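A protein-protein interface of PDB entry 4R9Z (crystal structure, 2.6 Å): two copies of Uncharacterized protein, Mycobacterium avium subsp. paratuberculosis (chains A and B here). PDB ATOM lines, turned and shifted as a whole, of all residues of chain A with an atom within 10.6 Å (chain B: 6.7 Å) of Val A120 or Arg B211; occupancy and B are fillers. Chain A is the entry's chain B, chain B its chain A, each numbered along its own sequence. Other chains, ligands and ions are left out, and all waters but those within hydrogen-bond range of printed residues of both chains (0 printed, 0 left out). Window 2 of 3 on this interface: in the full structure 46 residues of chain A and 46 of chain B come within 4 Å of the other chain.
OG of Ser B245 is in hydrogen-bond range of O of Val A120 (2.9 Å). The backbone NH (N) of Ser B245 is in hydrogen-bond range of the backbone carbonyl oxygen (O) of Tyr A122, at 3.0 Å. NE2 of His A227 lies within hydrogen-bond range of O of Ser B245, 3.4 Å away. OG of Ser B248 lies within hydrogen-bond range of NZ of Lys A111 (2.5 Å). O of Gly B247 sits close to O of Val A120, at 3.5 Å.
The side-chain hydroxyl (OG) of Ser B245 sits at hydrogen-bond distance from the guanidinium group (NH1) of Arg B211, 3.0 Å away. The backbone carbonyl oxygen (O) of Gly B247 sits at hydrogen-bond distance from the guanidinium group (NH2) of Arg B211 (2.6 Å). The side-chain hydroxyl of Ser B245 sits at hydrogen-bond distance from the backbone carbonyl oxygen of Gly B247 (3.2 Å). O of Ser B248 sits at hydrogen-bond distance from N of Phe B273, 2.7 Å away.
Among the printed residues, merely in contact across the chains: Tyr A122 with Ala B210 (3.3 Å), Tyr A122 with Ser B244 (3.4 Å), Val A121 with Ser B245 (3.4 Å), His A227 with Ala B246 (3.4 Å), Tyr A122 with Pro B170 (3.6 Å), Lys A111 with Leu B249 (3.7 Å), Val A120 with Arg B211 (3.8 Å), Val A121 with Gly B247 (3.9 Å) and His A227 with Ser B244 (3.9 Å).
Of chain B, only Arg B211, Ser B245 and Gly B247 come within 4 Å of Val A120. Of the printed residues of chain B, Val A121 touches Ser B245 and Gly B247. Thr B168 touches none of the printed residues of chain A. Of the printed residues of chain A, Pro B170 touches Tyr A122 (3.6 Å). Printed residues of chain A within 4 Å of Ala B210: Tyr A122 (3.3 Å). Arg B211 touches just one residue of chain A: Val A120. No residue of chain A comes within 4 Å of Gly B212. Gly B215 touches none of the printed residues of chain A. Printed residues of chain A within 4 Å of Ser B244: Tyr A122 and His A227. Of chain A, only Val A120, Val A121, Tyr A122 and His A227 come within 4 Å of Ser B245. Of the printed residues of chain A, Ala B246 touches His A227 (3.4 Å). Of the printed residues of chain A, Leu B249 touches Lys A111 (3.7 Å). The nearest residue of chain B that does not touch Val A120 is Ala B246 (4.8 Å). The nearest residue of chain A that does not touch Arg B211 is Gln A119 (4.7 Å). The nearest printed residue of chain A that does not touch Pro B170 is Gln A123 (5.9 Å).
Of the 8 printed residues of chain A, 5 touch a printed residue of chain B. Printed residues of chain B that touch a printed residue of chain A: Pro B170, Ala B210, Arg B211, Ser B244, Ser B245, Ala B246, Gly B247, Ser B248 and Leu B249. Among the printed residues, no Asp or Glu carboxylate lies within 4 Å of a Lys or Arg side-chain nitrogen of the other chain.
No position is printed for both chains. Of the 14 pairs that touch across the chains among the printed residues, none has its exchanged pair printed and touching as well.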
ATOM      1  N   LYS A 111     -21.384   9.497  -5.611  1.00  0.00           N
ATOM      2  CA  LYS A 111     -21.217  10.913  -5.320  1.00  0.00           C
ATOM      3  C   LYS A 111     -22.529  11.669  -5.462  1.00  0.00           C
ATOM      4  O   LYS A 111     -23.515  11.135  -5.973  1.00  0.00           O
ATOM      5  CB  LYS A 111     -20.154  11.539  -6.220  1.00  0.00           C
ATOM      6  CG  LYS A 111     -20.458  11.462  -7.695  1.00  0.00           C
ATOM      7  CD  LYS A 111     -19.436  12.257  -8.491  1.00  0.00           C
ATOM      8  CE  LYS A 111     -19.437  13.717  -8.075  1.00  0.00           C
ATOM      9  NZ  LYS A 111     -19.076  14.608  -9.209  1.00  0.00           N
ATOM     10  N   ASN A 114     -24.418  17.054  -9.816  1.00  0.00           N
ATOM     11  CA  ASN A 114     -24.620  18.447 -10.211  1.00  0.00           C
ATOM     12  C   ASN A 114     -26.098  18.839 -10.210  1.00  0.00           C
ATOM     13  O   ASN A 114     -26.593  19.443  -9.257  1.00  0.00           O
ATOM     14  CB  ASN A 114     -24.018  18.681 -11.602  1.00  0.00           C
ATOM     15  CG  ASN A 114     -23.816  20.152 -11.923  1.00  0.00           C
ATOM     16  OD1 ASN A 114     -24.517  21.021 -11.403  1.00  0.00           O
ATOM     17  ND2 ASN A 114     -22.853  20.436 -12.791  1.00  0.00           N
ATOM     18  N   GLN A 119     -17.815  20.145 -15.216  1.00  0.00           N
ATOM     19  CA  GLN A 119     -18.595  20.309 -16.439  1.00  0.00           C
ATOM     20  C   GLN A 119     -17.755  20.346 -17.715  1.00  0.00           C
ATOM     21  O   GLN A 119     -17.772  21.324 -18.463  1.00  0.00           O
ATOM     22  CB  GLN A 119     -19.470  21.556 -16.346  1.00  0.00           C
ATOM     23  CG  GLN A 119     -20.693  21.352 -15.465  1.00  0.00           C
ATOM     24  CD  GLN A 119     -21.359  20.000 -15.706  1.00  0.00           C
ATOM     25  OE1 GLN A 119     -21.074  19.021 -15.016  1.00  0.00           O
ATOM     26  NE2 GLN A 119     -22.232  19.941 -16.707  1.00  0.00           N
ATOM     27  N   VAL A 120     -17.019  19.264 -17.939  1.00  0.00           N
ATOM     28  CA  VAL A 120     -16.408  18.990 -19.230  1.00  0.00           C
ATOM     29  C   VAL A 120     -16.915  17.631 -19.656  1.00  0.00           C
ATOM     30  O   VAL A 120     -16.568  16.619 -19.054  1.00  0.00           O
ATOM     31  CB  VAL A 120     -14.881  18.973 -19.178  1.00  0.00           C
ATOM     32  CG1 VAL A 120     -14.323  18.518 -20.520  1.00  0.00           C
ATOM     33  CG2 VAL A 120     -14.345  20.344 -18.797  1.00  0.00           C
ATOM     34  N   VAL A 121     -17.716  17.607 -20.713  1.00  0.00           N
ATOM     35  CA  VAL A 121     -18.418  16.391 -21.095  1.00  0.00           C
ATOM     36  C   VAL A 121     -18.135  15.977 -22.532  1.00  0.00           C
ATOM     37  O   VAL A 121     -18.191  16.788 -23.457  1.00  0.00           O
ATOM     38  CB  VAL A 121     -19.948  16.561 -20.918  1.00  0.00           C
ATOM     39  CG1 VAL A 121     -20.685  15.263 -21.222  1.00  0.00           C
ATOM     40  CG2 VAL A 121     -20.269  17.056 -19.521  1.00  0.00           C
ATOM     41  N   TYR A 122     -17.811  14.697 -22.694  1.00  0.00           N
ATOM     42  CA  TYR A 122     -17.649  14.075 -23.997  1.00  0.00           C
ATOM     43  C   TYR A 122     -17.896  12.583 -23.874  1.00  0.00           C
ATOM     44  O   TYR A 122     -17.878  12.035 -22.776  1.00  0.00           O
ATOM     45  CB  TYR A 122     -16.266  14.358 -24.586  1.00  0.00           C
ATOM     46  CG  TYR A 122     -15.097  14.037 -23.685  1.00  0.00           C
ATOM     47  CD1 TYR A 122     -14.601  12.742 -23.577  1.00  0.00           C
ATOM     48  CD2 TYR A 122     -14.469  15.040 -22.963  1.00  0.00           C
ATOM     49  CE1 TYR A 122     -13.522  12.458 -22.757  1.00  0.00           C
ATOM     50  CE2 TYR A 122     -13.395  14.766 -22.145  1.00  0.00           C
ATOM     51  CZ  TYR A 122     -12.925  13.476 -22.047  1.00  0.00           C
ATOM     52  OH  TYR A 122     -11.855  13.212 -21.227  1.00  0.00           O
ATOM     53  N   GLN A 123     -18.171  11.939 -24.999  1.00  0.00           N
ATOM     54  CA  GLN A 123     -18.495  10.521 -25.001  1.00  0.00           C
ATOM     55  C   GLN A 123     -18.153   9.921 -26.353  1.00  0.00           C
ATOM     56  O   GLN A 123     -17.957  10.657 -27.323  1.00  0.00           O
ATOM     57  CB  GLN A 123     -19.975  10.311 -24.680  1.00  0.00           C
ATOM     58  CG  GLN A 123     -20.915  11.035 -25.626  1.00  0.00           C
ATOM     59  CD  GLN A 123     -22.361  10.630 -25.431  1.00  0.00           C
ATOM     60  OE1 GLN A 123     -23.049  11.149 -24.553  1.00  0.00           O
ATOM     61  NE2 GLN A 123     -22.827   9.691 -26.242  1.00  0.00           N
ATOM     62  N   HIS A 227     -22.279   6.909 -16.667  1.00  0.00           N
ATOM     63  CA  HIS A 227     -22.026   8.170 -17.300  1.00  0.00           C
ATOM     64  C   HIS A 227     -23.207   9.095 -17.148  1.00  0.00           C
ATOM     65  O   HIS A 227     -23.129  10.115 -16.515  1.00  0.00           O
ATOM     66  CB  HIS A 227     -21.726   7.929 -18.758  1.00  0.00           C
ATOM     67  CG  HIS A 227     -21.291   9.137 -19.497  1.00  0.00           C
ATOM     68  ND1 HIS A 227     -22.157   9.916 -20.212  1.00  0.00           N
ATOM     69  CD2 HIS A 227     -20.077   9.684 -19.665  1.00  0.00           C
ATOM     70  CE1 HIS A 227     -21.500  10.905 -20.772  1.00  0.00           C
ATOM     71  NE2 HIS A 227     -20.234  10.786 -20.454  1.00  0.00           N
ATOM     72  N   THR B 168      -5.352  16.547 -28.386  1.00  0.00           N
ATOM     73  CA  THR B 168      -6.086  16.924 -27.182  1.00  0.00           C
ATOM     74  C   THR B 168      -7.603  16.743 -27.312  1.00  0.00           C
ATOM     75  O   THR B 168      -8.313  16.713 -26.311  1.00  0.00           O
ATOM     76  CB  THR B 168      -5.798  18.384 -26.789  1.00  0.00           C
ATOM     77  OG1 THR B 168      -6.305  19.262 -27.802  1.00  0.00           O
ATOM     78  CG2 THR B 168      -4.300  18.606 -26.627  1.00  0.00           C
ATOM     79  N   PRO B 170     -10.978  14.696 -27.757  1.00  0.00           N
ATOM     80  CA  PRO B 170     -11.438  13.338 -27.436  1.00  0.00           C
ATOM     81  C   PRO B 170     -11.666  12.476 -28.683  1.00  0.00           C
ATOM     82  O   PRO B 170     -12.108  13.000 -29.707  1.00  0.00           O
ATOM     83  CB  PRO B 170     -12.751  13.591 -26.690  1.00  0.00           C
ATOM     84  CG  PRO B 170     -12.518  14.907 -26.015  1.00  0.00           C
ATOM     85  CD  PRO B 170     -11.736  15.718 -27.010  1.00  0.00           C
ATOM     86  N   PRO B 206      -4.273  11.216 -20.936  1.00  0.00           N
ATOM     87  CA  PRO B 206      -5.292  11.291 -21.988  1.00  0.00           C
ATOM     88  C   PRO B 206      -6.463  12.161 -21.541  1.00  0.00           C
ATOM     89  O   PRO B 206      -7.023  12.920 -22.331  1.00  0.00           O
ATOM     90  CB  PRO B 206      -5.741   9.838 -22.138  1.00  0.00           C
ATOM     91  CG  PRO B 206      -5.499   9.234 -20.797  1.00  0.00           C
ATOM     92  CD  PRO B 206      -4.264   9.904 -20.264  1.00  0.00           C
ATOM     93  N   ALA B 207      -6.822  12.029 -20.270  1.00  0.00           N
ATOM     94  CA  ALA B 207      -7.983  12.688 -19.692  1.00  0.00           C
ATOM     95  C   ALA B 207      -7.662  14.160 -19.468  1.00  0.00           C
ATOM     96  O   ALA B 207      -8.457  15.045 -19.784  1.00  0.00           O
ATOM     97  CB  ALA B 207      -8.392  12.022 -18.398  1.00  0.00           C
ATOM     98  N   PHE B 208      -6.471  14.393 -18.923  1.00  0.00           N
ATOM     99  CA  PHE B 208      -5.924  15.725 -18.694  1.00  0.00           C
ATOM    100  C   PHE B 208      -5.788  16.496 -20.000  1.00  0.00           C
ATOM    101  O   PHE B 208      -6.124  17.676 -20.072  1.00  0.00           O
ATOM    102  CB  PHE B 208      -4.571  15.602 -17.986  1.00  0.00           C
ATOM    103  CG  PHE B 208      -3.955  16.915 -17.597  1.00  0.00           C
ATOM    104  CD1 PHE B 208      -4.549  17.721 -16.637  1.00  0.00           C
ATOM    105  CD2 PHE B 208      -2.752  17.321 -18.159  1.00  0.00           C
ATOM    106  CE1 PHE B 208      -3.970  18.928 -16.270  1.00  0.00           C
ATOM    107  CE2 PHE B 208      -2.165  18.522 -17.794  1.00  0.00           C
ATOM    108  CZ  PHE B 208      -2.775  19.326 -16.846  1.00  0.00           C
ATOM    109  N   ALA B 209      -5.310  15.815 -21.034  1.00  0.00           N
ATOM    110  CA  ALA B 209      -5.190  16.421 -22.352  1.00  0.00           C
ATOM    111  C   ALA B 209      -6.570  16.787 -22.891  1.00  0.00           C
ATOM    112  O   ALA B 209      -6.784  17.912 -23.342  1.00  0.00           O
ATOM    113  CB  ALA B 209      -4.470  15.485 -23.311  1.00  0.00           C
ATOM    114  N   ALA B 210      -7.498  15.833 -22.839  1.00  0.00           N
ATOM    115  CA  ALA B 210      -8.860  16.025 -23.340  1.00  0.00           C
ATOM    116  C   ALA B 210      -9.549  17.226 -22.698  1.00  0.00           C
ATOM    117  O   ALA B 210     -10.438  17.836 -23.293  1.00  0.00           O
ATOM    118  CB  ALA B 210      -9.682  14.772 -23.121  1.00  0.00           C
ATOM    119  N   ARG B 211      -9.156  17.539 -21.472  1.00  0.00           N
ATOM    120  CA  ARG B 211      -9.705  18.676 -20.744  1.00  0.00           C
ATOM    121  C   ARG B 211      -9.058  19.993 -21.179  1.00  0.00           C
ATOM    122  O   ARG B 211      -9.567  21.075 -20.882  1.00  0.00           O
ATOM    123  CB  ARG B 211      -9.545  18.466 -19.243  1.00  0.00           C
ATOM    124  CG  ARG B 211     -10.704  17.709 -18.628  1.00  0.00           C
ATOM    125  CD  ARG B 211     -10.576  17.648 -17.122  1.00  0.00           C
ATOM    126  NE  ARG B 211     -11.837  17.897 -16.427  1.00  0.00           N
ATOM    127  CZ  ARG B 211     -12.903  17.103 -16.478  1.00  0.00           C
ATOM    128  NH1 ARG B 211     -12.884  15.988 -17.193  1.00  0.00           N
ATOM    129  NH2 ARG B 211     -13.996  17.426 -15.802  1.00  0.00           N
ATOM    130  N   GLY B 212      -7.921  19.896 -21.861  1.00  0.00           N
ATOM    131  CA  GLY B 212      -7.171  21.072 -22.263  1.00  0.00           C
ATOM    132  C   GLY B 212      -5.962  21.331 -21.389  1.00  0.00           C
ATOM    133  O   GLY B 212      -5.218  22.291 -21.602  1.00  0.00           O
ATOM    134  N   GLY B 213      -5.766  20.472 -20.396  1.00  0.00           N
ATOM    135  CA  GLY B 213      -4.562  20.516 -19.590  1.00  0.00           C
ATOM    136  C   GLY B 213      -4.631  21.576 -18.514  1.00  0.00           C
ATOM    137  O   GLY B 213      -3.649  22.268 -18.249  1.00  0.00           O
ATOM    138  N   VAL B 214      -5.796  21.698 -17.888  1.00  0.00           N
ATOM    139  CA  VAL B 214      -6.003  22.708 -16.861  1.00  0.00           C
ATOM    140  C   VAL B 214      -6.378  22.069 -15.524  1.00  0.00           C
ATOM    141  O   VAL B 214      -5.853  22.452 -14.478  1.00  0.00           O
ATOM    142  CB  VAL B 214      -7.089  23.727 -17.301  1.00  0.00           C
ATOM    143  CG1 VAL B 214      -7.980  23.128 -18.385  1.00  0.00           C
ATOM    144  CG2 VAL B 214      -7.913  24.218 -16.110  1.00  0.00           C
ATOM    145  N   GLY B 215      -7.254  21.070 -15.563  1.00  0.00           N
ATOM    146  CA  GLY B 215      -7.797  20.487 -14.348  1.00  0.00           C
ATOM    147  C   GLY B 215      -6.850  19.664 -13.491  1.00  0.00           C
ATOM    148  O   GLY B 215      -6.187  18.750 -13.980  1.00  0.00           O
ATOM    149  N   ALA B 216      -6.781  20.004 -12.204  1.00  0.00           N
ATOM    150  CA  ALA B 216      -6.048  19.205 -11.226  1.00  0.00           C
ATOM    151  C   ALA B 216      -6.858  17.936 -10.972  1.00  0.00           C
ATOM    152  O   ALA B 216      -8.085  17.994 -10.938  1.00  0.00           O
ATOM    153  CB  ALA B 216      -5.835  19.978  -9.951  1.00  0.00           C
ATOM    154  N   SER B 244     -14.532   8.918 -22.481  1.00  0.00           N
ATOM    155  CA  SER B 244     -15.666   9.644 -21.927  1.00  0.00           C
ATOM    156  C   SER B 244     -15.332  10.437 -20.670  1.00  0.00           C
ATOM    157  O   SER B 244     -14.380  10.130 -19.954  1.00  0.00           O
ATOM    158  CB  SER B 244     -16.811   8.672 -21.638  1.00  0.00           C
ATOM    159  OG  SER B 244     -16.356   7.566 -20.879  1.00  0.00           O
ATOM    160  N   SER B 245     -16.121  11.479 -20.433  1.00  0.00           N
ATOM    161  CA  SER B 245     -16.056  12.261 -19.209  1.00  0.00           C
ATOM    162  C   SER B 245     -17.467  12.690 -18.837  1.00  0.00           C
ATOM    163  O   SER B 245     -18.130  13.371 -19.615  1.00  0.00           O
ATOM    164  CB  SER B 245     -15.152  13.483 -19.387  1.00  0.00           C
ATOM    165  OG  SER B 245     -15.078  14.260 -18.202  1.00  0.00           O
ATOM    166  N   ALA B 246     -17.940  12.277 -17.665  1.00  0.00           N
ATOM    167  CA  ALA B 246     -19.281  12.652 -17.226  1.00  0.00           C
ATOM    168  C   ALA B 246     -19.195  13.759 -16.194  1.00  0.00           C
ATOM    169  O   ALA B 246     -19.581  13.577 -15.041  1.00  0.00           O
ATOM    170  CB  ALA B 246     -20.015  11.458 -16.653  1.00  0.00           C
ATOM    171  N   GLY B 247     -18.683  14.910 -16.612  1.00  0.00           N
ATOM    172  CA  GLY B 247     -18.497  16.017 -15.701  1.00  0.00           C
ATOM    173  C   GLY B 247     -17.155  15.899 -15.011  1.00  0.00           C
ATOM    174  O   GLY B 247     -16.107  15.965 -15.654  1.00  0.00           O
ATOM    175  N   SER B 248     -17.194  15.694 -13.699  1.00  0.00           N
ATOM    176  CA  SER B 248     -15.984  15.629 -12.883  1.00  0.00           C
ATOM    177  C   SER B 248     -15.284  14.273 -12.985  1.00  0.00           C
ATOM    178  O   SER B 248     -14.120  14.137 -12.607  1.00  0.00           O
ATOM    179  CB  SER B 248     -16.321  15.939 -11.419  1.00  0.00           C
ATOM    180  OG  SER B 248     -17.446  15.190 -10.980  1.00  0.00           O
ATOM    181  N   LEU B 249     -16.004  13.274 -13.486  1.00  0.00           N
ATOM    182  CA  LEU B 249     -15.463  11.927 -13.615  1.00  0.00           C
ATOM    183  C   LEU B 249     -15.132  11.581 -15.068  1.00  0.00           C
ATOM    184  O   LEU B 249     -16.019  11.501 -15.921  1.00  0.00           O
ATOM    185  CB  LEU B 249     -16.454  10.912 -13.050  1.00  0.00           C
ATOM    186  CG  LEU B 249     -16.682  11.036 -11.545  1.00  0.00           C
ATOM    187  CD1 LEU B 249     -17.853  10.180 -11.103  1.00  0.00           C
ATOM    188  CD2 LEU B 249     -15.421  10.652 -10.791  1.00  0.00           C
ATOM    189  N   ALA B 250     -13.853  11.356 -15.342  1.00  0.00           N
ATOM    190  CA  ALA B 250     -13.424  10.980 -16.682  1.00  0.00           C
ATOM    191  C   ALA B 250     -12.936   9.542 -16.704  1.00  0.00           C
ATOM    192  O   ALA B 250     -12.267   9.082 -15.776  1.00  0.00           O
ATOM    193  CB  ALA B 250     -12.334  11.915 -17.178  1.00  0.00           C
ATOM    194  N   MET B 271     -11.077   8.827 -13.067  1.00  0.00           N
ATOM    195  CA  MET B 271     -10.419   9.849 -12.260  1.00  0.00           C
ATOM    196  C   MET B 271     -11.298  11.066 -12.034  1.00  0.00           C
ATOM    197  O   MET B 271     -12.157  11.397 -12.852  1.00  0.00           O
ATOM    198  CB  MET B 271      -9.104  10.265 -12.899  1.00  0.00           C
ATOM    199  CG  MET B 271      -9.266  10.952 -14.223  1.00  0.00           C
ATOM    200  SD  MET B 271      -7.774  10.738 -15.193  1.00  0.00           S
ATOM    201  CE  MET B 271      -7.984   9.044 -15.705  1.00  0.00           C
ATOM    202  N   TYR B 272     -11.075  11.712 -10.894  1.00  0.00           N
ATOM    203  CA  TYR B 272     -11.878  12.843 -10.456  1.00  0.00           C
ATOM    204  C   TYR B 272     -11.189  14.172 -10.737  1.00  0.00           C
ATOM    205  O   TYR B 272     -10.037  14.386 -10.350  1.00  0.00           O
ATOM    206  CB  TYR B 272     -12.176  12.712  -8.958  1.00  0.00           C
ATOM    207  CG  TYR B 272     -12.967  13.847  -8.337  1.00  0.00           C
ATOM    208  CD1 TYR B 272     -14.267  14.125  -8.743  1.00  0.00           C
ATOM    209  CD2 TYR B 272     -12.416  14.631  -7.328  1.00  0.00           C
ATOM    210  CE1 TYR B 272     -14.993  15.154  -8.163  1.00  0.00           C
ATOM    211  CE2 TYR B 272     -13.133  15.658  -6.743  1.00  0.00           C
ATOM    212  CZ  TYR B 272     -14.419  15.919  -7.166  1.00  0.00           C
ATOM    213  OH  TYR B 272     -15.137  16.944  -6.590  1.00  0.00           O
ATOM    214  N   PHE B 273     -11.910  15.062 -11.415  1.00  0.00           N
ATOM    215  CA  PHE B 273     -11.460  16.433 -11.624  1.00  0.00           C
ATOM    216  C   PHE B 273     -12.351  17.392 -10.852  1.00  0.00           C
ATOM    217  O   PHE B 273     -13.484  17.640 -11.262  1.00  0.00           O
ATOM    218  CB  PHE B 273     -11.484  16.800 -13.109  1.00  0.00           C
ATOM    219  CG  PHE B 273     -10.405  16.146 -13.913  1.00  0.00           C
ATOM    220  CD1 PHE B 273     -10.616  14.908 -14.497  1.00  0.00           C
ATOM    221  CD2 PHE B 273      -9.179  16.765 -14.082  1.00  0.00           C
ATOM    222  CE1 PHE B 273      -9.629  14.306 -15.235  1.00  0.00           C
ATOM    223  CE2 PHE B 273      -8.188  16.166 -14.825  1.00  0.00           C
ATOM    224  CZ  PHE B 273      -8.410  14.935 -15.398  1.00  0.00           C
ATOM    225  N   PRO B 274     -11.845  17.925  -9.729  1.00  0.00           N
ATOM    226  CA  PRO B 274     -12.582  18.904  -8.924  1.00  0.00           C
ATOM    227  C   PRO B 274     -12.863  20.179  -9.711  1.00  0.00           C
ATOM    228  O   PRO B 274     -11.954  20.690 -10.364  1.00  0.00           O
ATOM    229  CB  PRO B 274     -11.637  19.188  -7.754  1.00  0.00           C
ATOM    230  CG  PRO B 274     -10.720  18.034  -7.698  1.00  0.00           C
ATOM    231  CD  PRO B 274     -10.572  17.539  -9.102  1.00  0.00           C
